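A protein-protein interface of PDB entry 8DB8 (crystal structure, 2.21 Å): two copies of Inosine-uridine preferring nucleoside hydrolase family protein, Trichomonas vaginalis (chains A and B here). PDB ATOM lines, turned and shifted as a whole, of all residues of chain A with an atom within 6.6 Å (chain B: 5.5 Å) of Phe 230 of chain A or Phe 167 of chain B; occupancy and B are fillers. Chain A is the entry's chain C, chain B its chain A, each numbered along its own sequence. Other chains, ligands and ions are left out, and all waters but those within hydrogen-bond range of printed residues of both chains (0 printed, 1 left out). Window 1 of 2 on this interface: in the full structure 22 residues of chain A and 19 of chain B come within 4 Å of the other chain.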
ATOM      1  N   LYS A 225      -7.934 -19.201 -33.161  1.00  0.00           N
ATOM      2  CA  LYS A 225      -6.680 -18.802 -32.525  1.00  0.00           C
ATOM      3  C   LYS A 225      -6.881 -17.771 -31.413  1.00  0.00           C
ATOM      4  O   LYS A 225      -6.420 -18.004 -30.287  1.00  0.00           O
ATOM      5  CB  LYS A 225      -5.691 -18.271 -33.571  1.00  0.00           C
ATOM      6  CG  LYS A 225      -4.373 -17.794 -32.990  1.00  0.00           C
ATOM      7  CD  LYS A 225      -3.421 -17.323 -34.081  1.00  0.00           C
ATOM      8  CE  LYS A 225      -2.112 -16.823 -33.486  1.00  0.00           C
ATOM      9  NZ  LYS A 225      -1.194 -16.283 -34.524  1.00  0.00           N
ATOM     10  N   PRO A 226      -7.541 -16.632 -31.657  1.00  0.00           N
ATOM     11  CA  PRO A 226      -7.703 -15.657 -30.565  1.00  0.00           C
ATOM     12  C   PRO A 226      -8.607 -16.147 -29.446  1.00  0.00           C
ATOM     13  O   PRO A 226      -8.466 -15.680 -28.309  1.00  0.00           O
ATOM     14  CB  PRO A 226      -8.287 -14.425 -31.270  1.00  0.00           C
ATOM     15  CG  PRO A 226      -8.933 -14.953 -32.486  1.00  0.00           C
ATOM     16  CD  PRO A 226      -8.132 -16.136 -32.916  1.00  0.00           C
ATOM     17  N   ILE A 227      -9.531 -17.069 -29.728  1.00  0.00           N
ATOM     18  CA  ILE A 227     -10.323 -17.671 -28.660  1.00  0.00           C
ATOM     19  C   ILE A 227      -9.432 -18.500 -27.746  1.00  0.00           C
ATOM     20  O   ILE A 227      -9.461 -18.350 -26.517  1.00  0.00           O
ATOM     21  CB  ILE A 227     -11.461 -18.526 -29.244  1.00  0.00           C
ATOM     22  CG1 ILE A 227     -12.513 -17.643 -29.910  1.00  0.00           C
ATOM     23  CG2 ILE A 227     -12.083 -19.379 -28.147  1.00  0.00           C
ATOM     24  CD1 ILE A 227     -13.093 -16.588 -28.993  1.00  0.00           C
ATOM     25  N   ILE A 228      -8.636 -19.395 -28.336  1.00  0.00           N
ATOM     26  CA  ILE A 228      -7.734 -20.233 -27.552  1.00  0.00           C
ATOM     27  C   ILE A 228      -6.736 -19.375 -26.790  1.00  0.00           C
ATOM     28  O   ILE A 228      -6.387 -19.672 -25.641  1.00  0.00           O
ATOM     29  CB  ILE A 228      -7.024 -21.238 -28.474  1.00  0.00           C
ATOM     30  CG1 ILE A 228      -8.009 -22.289 -28.985  1.00  0.00           C
ATOM     31  CG2 ILE A 228      -5.859 -21.896 -27.763  1.00  0.00           C
ATOM     32  CD1 ILE A 228      -7.425 -23.194 -30.044  1.00  0.00           C
ATOM     33  N   ALA A 229      -6.279 -18.285 -27.411  1.00  0.00           N
ATOM     34  CA  ALA A 229      -5.216 -17.480 -26.823  1.00  0.00           C
ATOM     35  C   ALA A 229      -5.713 -16.676 -25.626  1.00  0.00           C
ATOM     36  O   ALA A 229      -4.999 -16.536 -24.626  1.00  0.00           O
ATOM     37  CB  ALA A 229      -4.623 -16.553 -27.884  1.00  0.00           C
ATOM     38  N   PHE A 230      -6.931 -16.145 -25.704  1.00  0.00           N
ATOM     39  CA  PHE A 230      -7.448 -15.249 -24.678  1.00  0.00           C
ATOM     40  C   PHE A 230      -8.357 -15.942 -23.671  1.00  0.00           C
ATOM     41  O   PHE A 230      -8.859 -15.280 -22.756  1.00  0.00           O
ATOM     42  CB  PHE A 230      -8.196 -14.078 -25.328  1.00  0.00           C
ATOM     43  CG  PHE A 230      -7.292 -13.027 -25.909  1.00  0.00           C
ATOM     44  CD1 PHE A 230      -6.790 -12.008 -25.113  1.00  0.00           C
ATOM     45  CD2 PHE A 230      -6.945 -13.056 -27.250  1.00  0.00           C
ATOM     46  CE1 PHE A 230      -5.959 -11.038 -25.645  1.00  0.00           C
ATOM     47  CE2 PHE A 230      -6.113 -12.091 -27.787  1.00  0.00           C
ATOM     48  CZ  PHE A 230      -5.618 -11.082 -26.983  1.00  0.00           C
ATOM     49  N   ASP A 231      -8.579 -17.248 -23.809  1.00  0.00           N
ATOM     50  CA  ASP A 231      -9.424 -17.993 -22.884  1.00  0.00           C
ATOM     51  C   ASP A 231      -8.658 -19.134 -22.222  1.00  0.00           C
ATOM     52  O   ASP A 231      -9.231 -20.185 -21.924  1.00  0.00           O
ATOM     53  CB  ASP A 231     -10.668 -18.526 -23.594  1.00  0.00           C
ATOM     54  CG  ASP A 231     -11.854 -18.683 -22.658  1.00  0.00           C
ATOM     55  OD1 ASP A 231     -11.640 -18.745 -21.429  1.00  0.00           O
ATOM     56  OD2 ASP A 231     -13.000 -18.756 -23.154  1.00  0.00           O
ATOM     57  N   GLY A 232      -7.361 -18.943 -21.991  1.00  0.00           N
ATOM     58  CA  GLY A 232      -6.579 -19.956 -21.308  1.00  0.00           C
ATOM     59  C   GLY A 232      -6.439 -21.263 -22.050  1.00  0.00           C
ATOM     60  O   GLY A 232      -6.102 -22.280 -21.439  1.00  0.00           O
ATOM     61  N   GLY A 233      -6.684 -21.266 -23.358  1.00  0.00           N
ATOM     62  CA  GLY A 233      -6.656 -22.476 -24.148  1.00  0.00           C
ATOM     63  C   GLY A 233      -7.989 -23.177 -24.278  1.00  0.00           C
ATOM     64  O   GLY A 233      -8.056 -24.227 -24.932  1.00  0.00           O
ATOM     65  N   ASP B   8      -6.512  -8.333 -10.770  1.00  0.00           N
ATOM     66  CA  ASP B   8      -7.787  -8.235 -11.467  1.00  0.00           C
ATOM     67  C   ASP B   8      -8.753  -9.188 -10.781  1.00  0.00           C
ATOM     68  O   ASP B   8      -9.457  -9.958 -11.446  1.00  0.00           O
ATOM     69  CB  ASP B   8      -7.639  -8.583 -12.948  1.00  0.00           C
ATOM     70  CG  ASP B   8      -6.875  -9.877 -13.171  1.00  0.00           C
ATOM     71  OD1 ASP B   8      -6.409 -10.474 -12.181  1.00  0.00           O
ATOM     72  OD2 ASP B   8      -6.738 -10.299 -14.338  1.00  0.00           O
ATOM     73  N   GLY B  36     -10.054  -4.964 -17.346  1.00  0.00           N
ATOM     74  CA  GLY B  36      -9.715  -5.874 -18.426  1.00  0.00           C
ATOM     75  C   GLY B  36     -10.694  -7.028 -18.525  1.00  0.00           C
ATOM     76  O   GLY B  36     -11.852  -6.831 -18.893  1.00  0.00           O
ATOM     77  N   ASN B  37     -10.230  -8.233 -18.205  1.00  0.00           N
ATOM     78  CA  ASN B  37     -11.080  -9.420 -18.245  1.00  0.00           C
ATOM     79  C   ASN B  37     -12.297  -9.181 -17.364  1.00  0.00           C
ATOM     80  O   ASN B  37     -13.435  -9.199 -17.833  1.00  0.00           O
ATOM     81  CB  ASN B  37     -10.310 -10.651 -17.766  1.00  0.00           C
ATOM     82  CG  ASN B  37     -11.223 -11.814 -17.431  1.00  0.00           C
ATOM     83  OD1 ASN B  37     -12.382 -11.848 -17.844  1.00  0.00           O
ATOM     84  ND2 ASN B  37     -10.703 -12.777 -16.678  1.00  0.00           N
ATOM     85  N   MET B  74     -11.286  -7.266 -25.584  1.00  0.00           N
ATOM     86  CA  MET B  74     -11.664  -8.537 -26.195  1.00  0.00           C
ATOM     87  C   MET B  74     -12.696  -9.241 -25.317  1.00  0.00           C
ATOM     88  O   MET B  74     -12.321  -9.993 -24.409  1.00  0.00           O
ATOM     89  CB  MET B  74     -10.412  -9.404 -26.415  1.00  0.00           C
ATOM     90  CG  MET B  74     -10.674 -10.769 -27.025  1.00  0.00           C
ATOM     91  SD  MET B  74     -11.518 -10.673 -28.610  1.00  0.00           S
ATOM     92  CE  MET B  74     -10.118 -10.629 -29.707  1.00  0.00           C
ATOM     93  N   PRO B 127      -2.890  -8.034 -15.795  1.00  0.00           N
ATOM     94  CA  PRO B 127      -2.204  -7.205 -16.790  1.00  0.00           C
ATOM     95  C   PRO B 127      -1.551  -6.002 -16.127  1.00  0.00           C
ATOM     96  O   PRO B 127      -2.084  -5.427 -15.175  1.00  0.00           O
ATOM     97  CB  PRO B 127      -3.331  -6.794 -17.742  1.00  0.00           C
ATOM     98  CG  PRO B 127      -4.271  -7.952 -17.691  1.00  0.00           C
ATOM     99  CD  PRO B 127      -4.213  -8.478 -16.274  1.00  0.00           C
ATOM    100  N   GLY B 165      -2.772 -20.056 -24.230  1.00  0.00           N
ATOM    101  CA  GLY B 165      -3.699 -19.503 -23.267  1.00  0.00           C
ATOM    102  C   GLY B 165      -3.135 -18.553 -22.234  1.00  0.00           C
ATOM    103  O   GLY B 165      -3.857 -18.202 -21.293  1.00  0.00           O
ATOM    104  N   GLU B 166      -1.881 -18.129 -22.367  1.00  0.00           N
ATOM    105  CA  GLU B 166      -1.359 -17.106 -21.471  1.00  0.00           C
ATOM    106  C   GLU B 166      -2.223 -15.855 -21.581  1.00  0.00           C
ATOM    107  O   GLU B 166      -2.645 -15.468 -22.677  1.00  0.00           O
ATOM    108  CB  GLU B 166       0.100 -16.789 -21.817  1.00  0.00           C
ATOM    109  CG  GLU B 166       0.826 -15.917 -20.799  1.00  0.00           C
ATOM    110  CD  GLU B 166       0.459 -14.452 -20.919  1.00  0.00           C
ATOM    111  OE1 GLU B 166       0.169 -14.012 -22.049  1.00  0.00           O
ATOM    112  OE2 GLU B 166       0.458 -13.742 -19.890  1.00  0.00           O
ATOM    113  N   PHE B 167      -2.502 -15.221 -20.443  1.00  0.00           N
ATOM    114  CA  PHE B 167      -3.484 -14.142 -20.426  1.00  0.00           C
ATOM    115  C   PHE B 167      -2.905 -12.787 -20.053  1.00  0.00           C
ATOM    116  O   PHE B 167      -3.135 -11.808 -20.773  1.00  0.00           O
ATOM    117  CB  PHE B 167      -4.636 -14.475 -19.464  1.00  0.00           C
ATOM    118  CG  PHE B 167      -5.681 -13.402 -19.408  1.00  0.00           C
ATOM    119  CD1 PHE B 167      -6.581 -13.244 -20.448  1.00  0.00           C
ATOM    120  CD2 PHE B 167      -5.738 -12.525 -18.337  1.00  0.00           C
ATOM    121  CE1 PHE B 167      -7.534 -12.247 -20.414  1.00  0.00           C
ATOM    122  CE2 PHE B 167      -6.687 -11.523 -18.298  1.00  0.00           C
ATOM    123  CZ  PHE B 167      -7.588 -11.383 -19.337  1.00  0.00           C
ATOM    124  N   ASN B 168      -2.167 -12.695 -18.942  1.00  0.00           N
ATOM    125  CA  ASN B 168      -1.861 -11.395 -18.346  1.00  0.00           C
ATOM    126  C   ASN B 168      -1.107 -10.490 -19.314  1.00  0.00           C
ATOM    127  O   ASN B 168      -1.472  -9.323 -19.505  1.00  0.00           O
ATOM    128  CB  ASN B 168      -1.055 -11.588 -17.060  1.00  0.00           C
ATOM    129  CG  ASN B 168      -1.934 -11.853 -15.854  1.00  0.00           C
ATOM    130  OD1 ASN B 168      -3.155 -11.703 -15.911  1.00  0.00           O
ATOM    131  ND2 ASN B 168      -1.312 -12.241 -14.747  1.00  0.00           N
ATOM    132  N   TRP B 169      -0.048 -11.005 -19.931  1.00  0.00           N
ATOM    133  CA  TRP B 169       0.764 -10.155 -20.793  1.00  0.00           C
ATOM    134  C   TRP B 169       0.137 -10.004 -22.173  1.00  0.00           C
ATOM    135  O   TRP B 169       0.212  -8.932 -22.782  1.00  0.00           O
ATOM    136  CB  TRP B 169       2.177 -10.722 -20.893  1.00  0.00           C
ATOM    137  CG  TRP B 169       2.922 -10.646 -19.593  1.00  0.00           C
ATOM    138  CD1 TRP B 169       2.447 -10.183 -18.399  1.00  0.00           C
ATOM    139  CD2 TRP B 169       4.277 -11.041 -19.356  1.00  0.00           C
ATOM    140  NE1 TRP B 169       3.420 -10.268 -17.434  1.00  0.00           N
ATOM    141  CE2 TRP B 169       4.555 -10.793 -17.995  1.00  0.00           C
ATOM    142  CE3 TRP B 169       5.286 -11.582 -20.162  1.00  0.00           C
ATOM    143  CZ2 TRP B 169       5.794 -11.068 -17.423  1.00  0.00           C
ATOM    144  CZ3 TRP B 169       6.515 -11.856 -19.591  1.00  0.00           C
ATOM    145  CH2 TRP B 169       6.758 -11.598 -18.234  1.00  0.00           C
ATOM    146  N   ARG B 170      -0.492 -11.066 -22.671  1.00  0.00           N
ATOM    147  CA  ARG B 170      -1.212 -10.987 -23.935  1.00  0.00           C
ATOM    148  C   ARG B 170      -2.340  -9.960 -23.877  1.00  0.00           C
ATOM    149  O   ARG B 170      -2.663  -9.331 -24.893  1.00  0.00           O
ATOM    150  CB  ARG B 170      -1.743 -12.377 -24.281  1.00  0.00           C
ATOM    151  CG  ARG B 170      -2.712 -12.445 -25.424  1.00  0.00           C
ATOM    152  CD  ARG B 170      -3.088 -13.890 -25.672  1.00  0.00           C
ATOM    153  NE  ARG B 170      -2.262 -14.484 -26.716  1.00  0.00           N
ATOM    154  CZ  ARG B 170      -1.587 -15.622 -26.586  1.00  0.00           C
ATOM    155  NH1 ARG B 170      -1.638 -16.307 -25.450  1.00  0.00           N
ATOM    156  NH2 ARG B 170      -0.867 -16.081 -27.603  1.00  0.00           N
ATOM    157  N   ALA B 171      -2.930  -9.755 -22.694  1.00  0.00           N
ATOM    158  CA  ALA B 171      -4.032  -8.805 -22.561  1.00  0.00           C
ATOM    159  C   ALA B 171      -3.565  -7.361 -22.707  1.00  0.00           C
ATOM    160  O   ALA B 171      -4.311  -6.524 -23.225  1.00  0.00           O
ATOM    161  CB  ALA B 171      -4.736  -8.999 -21.219  1.00  0.00           C
ATOM    162  N   ASP B 172      -2.353  -7.042 -22.252  1.00  0.00           N
ATOM    163  CA  ASP B 172      -1.758  -5.718 -22.451  1.00  0.00           C
ATOM    164  C   ASP B 172      -0.281  -5.894 -22.762  1.00  0.00           C
ATOM    165  O   ASP B 172       0.585  -5.696 -21.901  1.00  0.00           O
ATOM    166  CB  ASP B 172      -1.967  -4.821 -21.227  1.00  0.00           C
ATOM    167  CG  ASP B 172      -1.814  -3.342 -21.554  1.00  0.00           C
ATOM    168  OD1 ASP B 172      -1.164  -3.020 -22.570  1.00  0.00           O
ATOM    169  OD2 ASP B 172      -2.341  -2.499 -20.795  1.00  0.00           O
ATOM    170  N   TRP B 193       2.875 -18.710 -17.064  1.00  0.00           N
ATOM    171  CA  TRP B 193       1.788 -19.602 -17.458  1.00  0.00           C
ATOM    172  C   TRP B 193       2.308 -20.997 -17.768  1.00  0.00           C
ATOM    173  O   TRP B 193       1.588 -21.984 -17.580  1.00  0.00           O
ATOM    174  CB  TRP B 193       1.043 -19.025 -18.664  1.00  0.00           C
ATOM    175  CG  TRP B 193      -0.130 -19.855 -19.117  1.00  0.00           C
ATOM    176  CD1 TRP B 193      -0.320 -20.396 -20.357  1.00  0.00           C
ATOM    177  CD2 TRP B 193      -1.274 -20.231 -18.339  1.00  0.00           C
ATOM    178  NE1 TRP B 193      -1.508 -21.086 -20.400  1.00  0.00           N
ATOM    179  CE2 TRP B 193      -2.113 -21.001 -19.172  1.00  0.00           C
ATOM    180  CE3 TRP B 193      -1.671 -19.993 -17.020  1.00  0.00           C
ATOM    181  CZ2 TRP B 193      -3.324 -21.535 -18.728  1.00  0.00           C
ATOM    182  CZ3 TRP B 193      -2.875 -20.525 -16.580  1.00  0.00           C
ATOM    183  CH2 TRP B 193      -3.686 -21.286 -17.433  1.00  0.00           C
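O of Ala 229 of chain A lies close to NH1 of Arg 170 of chain B, at 3.5 Å. The backbone carbonyl oxygen (O) of Ala 229 of chain A sits close to the backbone carbonyl oxygen (O) of Glu 166 of chain B (3.2 Å).
The backbone NH (N) of Asn 168 of chain B lies within hydrogen-bond range of the side-chain carboxylate (OE2) of Glu 166 of chain B, at 3.0 Å. OE2 of Glu 166 of chain B lies within hydrogen-bond range of N of Trp 169 of chain B (2.8 Å). O of Glu 166 of chain B sits at hydrogen-bond distance from NH1 of Arg 170 of chain B, at 3.1 Å. The backbone carbonyl oxygen (O) of Ile 228 of chain A lies within hydrogen-bond range of the backbone NH (N) of Gly 233 of chain A, 2.8 Å away.
Ile 228 of chain A touches Gly 165 of chain B. Gly 165 of chain B touches Ala 229 of chain A. CD1 of Phe 167 of chain B touches O of Phe 230 of chain A, 3.8 Å away. CE1 of Phe 230 of chain A touches CG of Arg 170 of chain B, 3.5 Å away. Gly 232 of chain A touches Gly 165 of chain B (CA to O, 3.2 Å). Gly 232 of chain A touches Trp 193 of chain B (O to CZ2, 3.95 Å). Gly 165 of chain B touches Gly 233 of chain A (CA to N, 3.5 Å).
Of chain B, only Phe 167 (3.8 Å) and Arg 170 (3.5 Å) come within 4 Å of Phe 230 of chain A. Of chain A, only Phe 230 (3.8 Å) comes within 4 Å of Phe 167 of chain B. Of the printed residues of chain B, Gly 233 of chain A touches Gly 165. Printed residues of chain B within 4 Å of Gly 232 of chain A: Gly 165 and Trp 193. Printed residues of chain B within 4 Å of Ala 229 of chain A: Gly 165 (3.5 Å), Glu 166 (3.2 Å) and Arg 170 (3.3 Å). Of the printed residues of chain A, Gly 165 of chain B touches Ile 228 (3.6 Å), Ala 229 (3.5 Å), Gly 232 (3.2 Å) and Gly 233 (3.5 Å). Printed residues of chain B within 4 Å of Ile 228 of chain A: Gly 165 (3.6 Å). Asp 172 of chain B touches none of the printed residues of chain A. Asn 168 of chain B touches none of the printed residues of chain A. The nearest residue of chain A that does not touch Phe 167 of chain B is Ala 229 of chain A (5.0 Å).
Of the 14 printed residues of chain B, 5 touch a printed residue of chain A. Printed residues of chain B that touch a printed residue of chain A: Gly 165, Glu 166, Phe 167, Arg 170 and Trp 193.
No position is printed for both chains. Of the 9 pairs that touch across the chains among the printed residues, none has its exchanged pair printed and touching as well.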
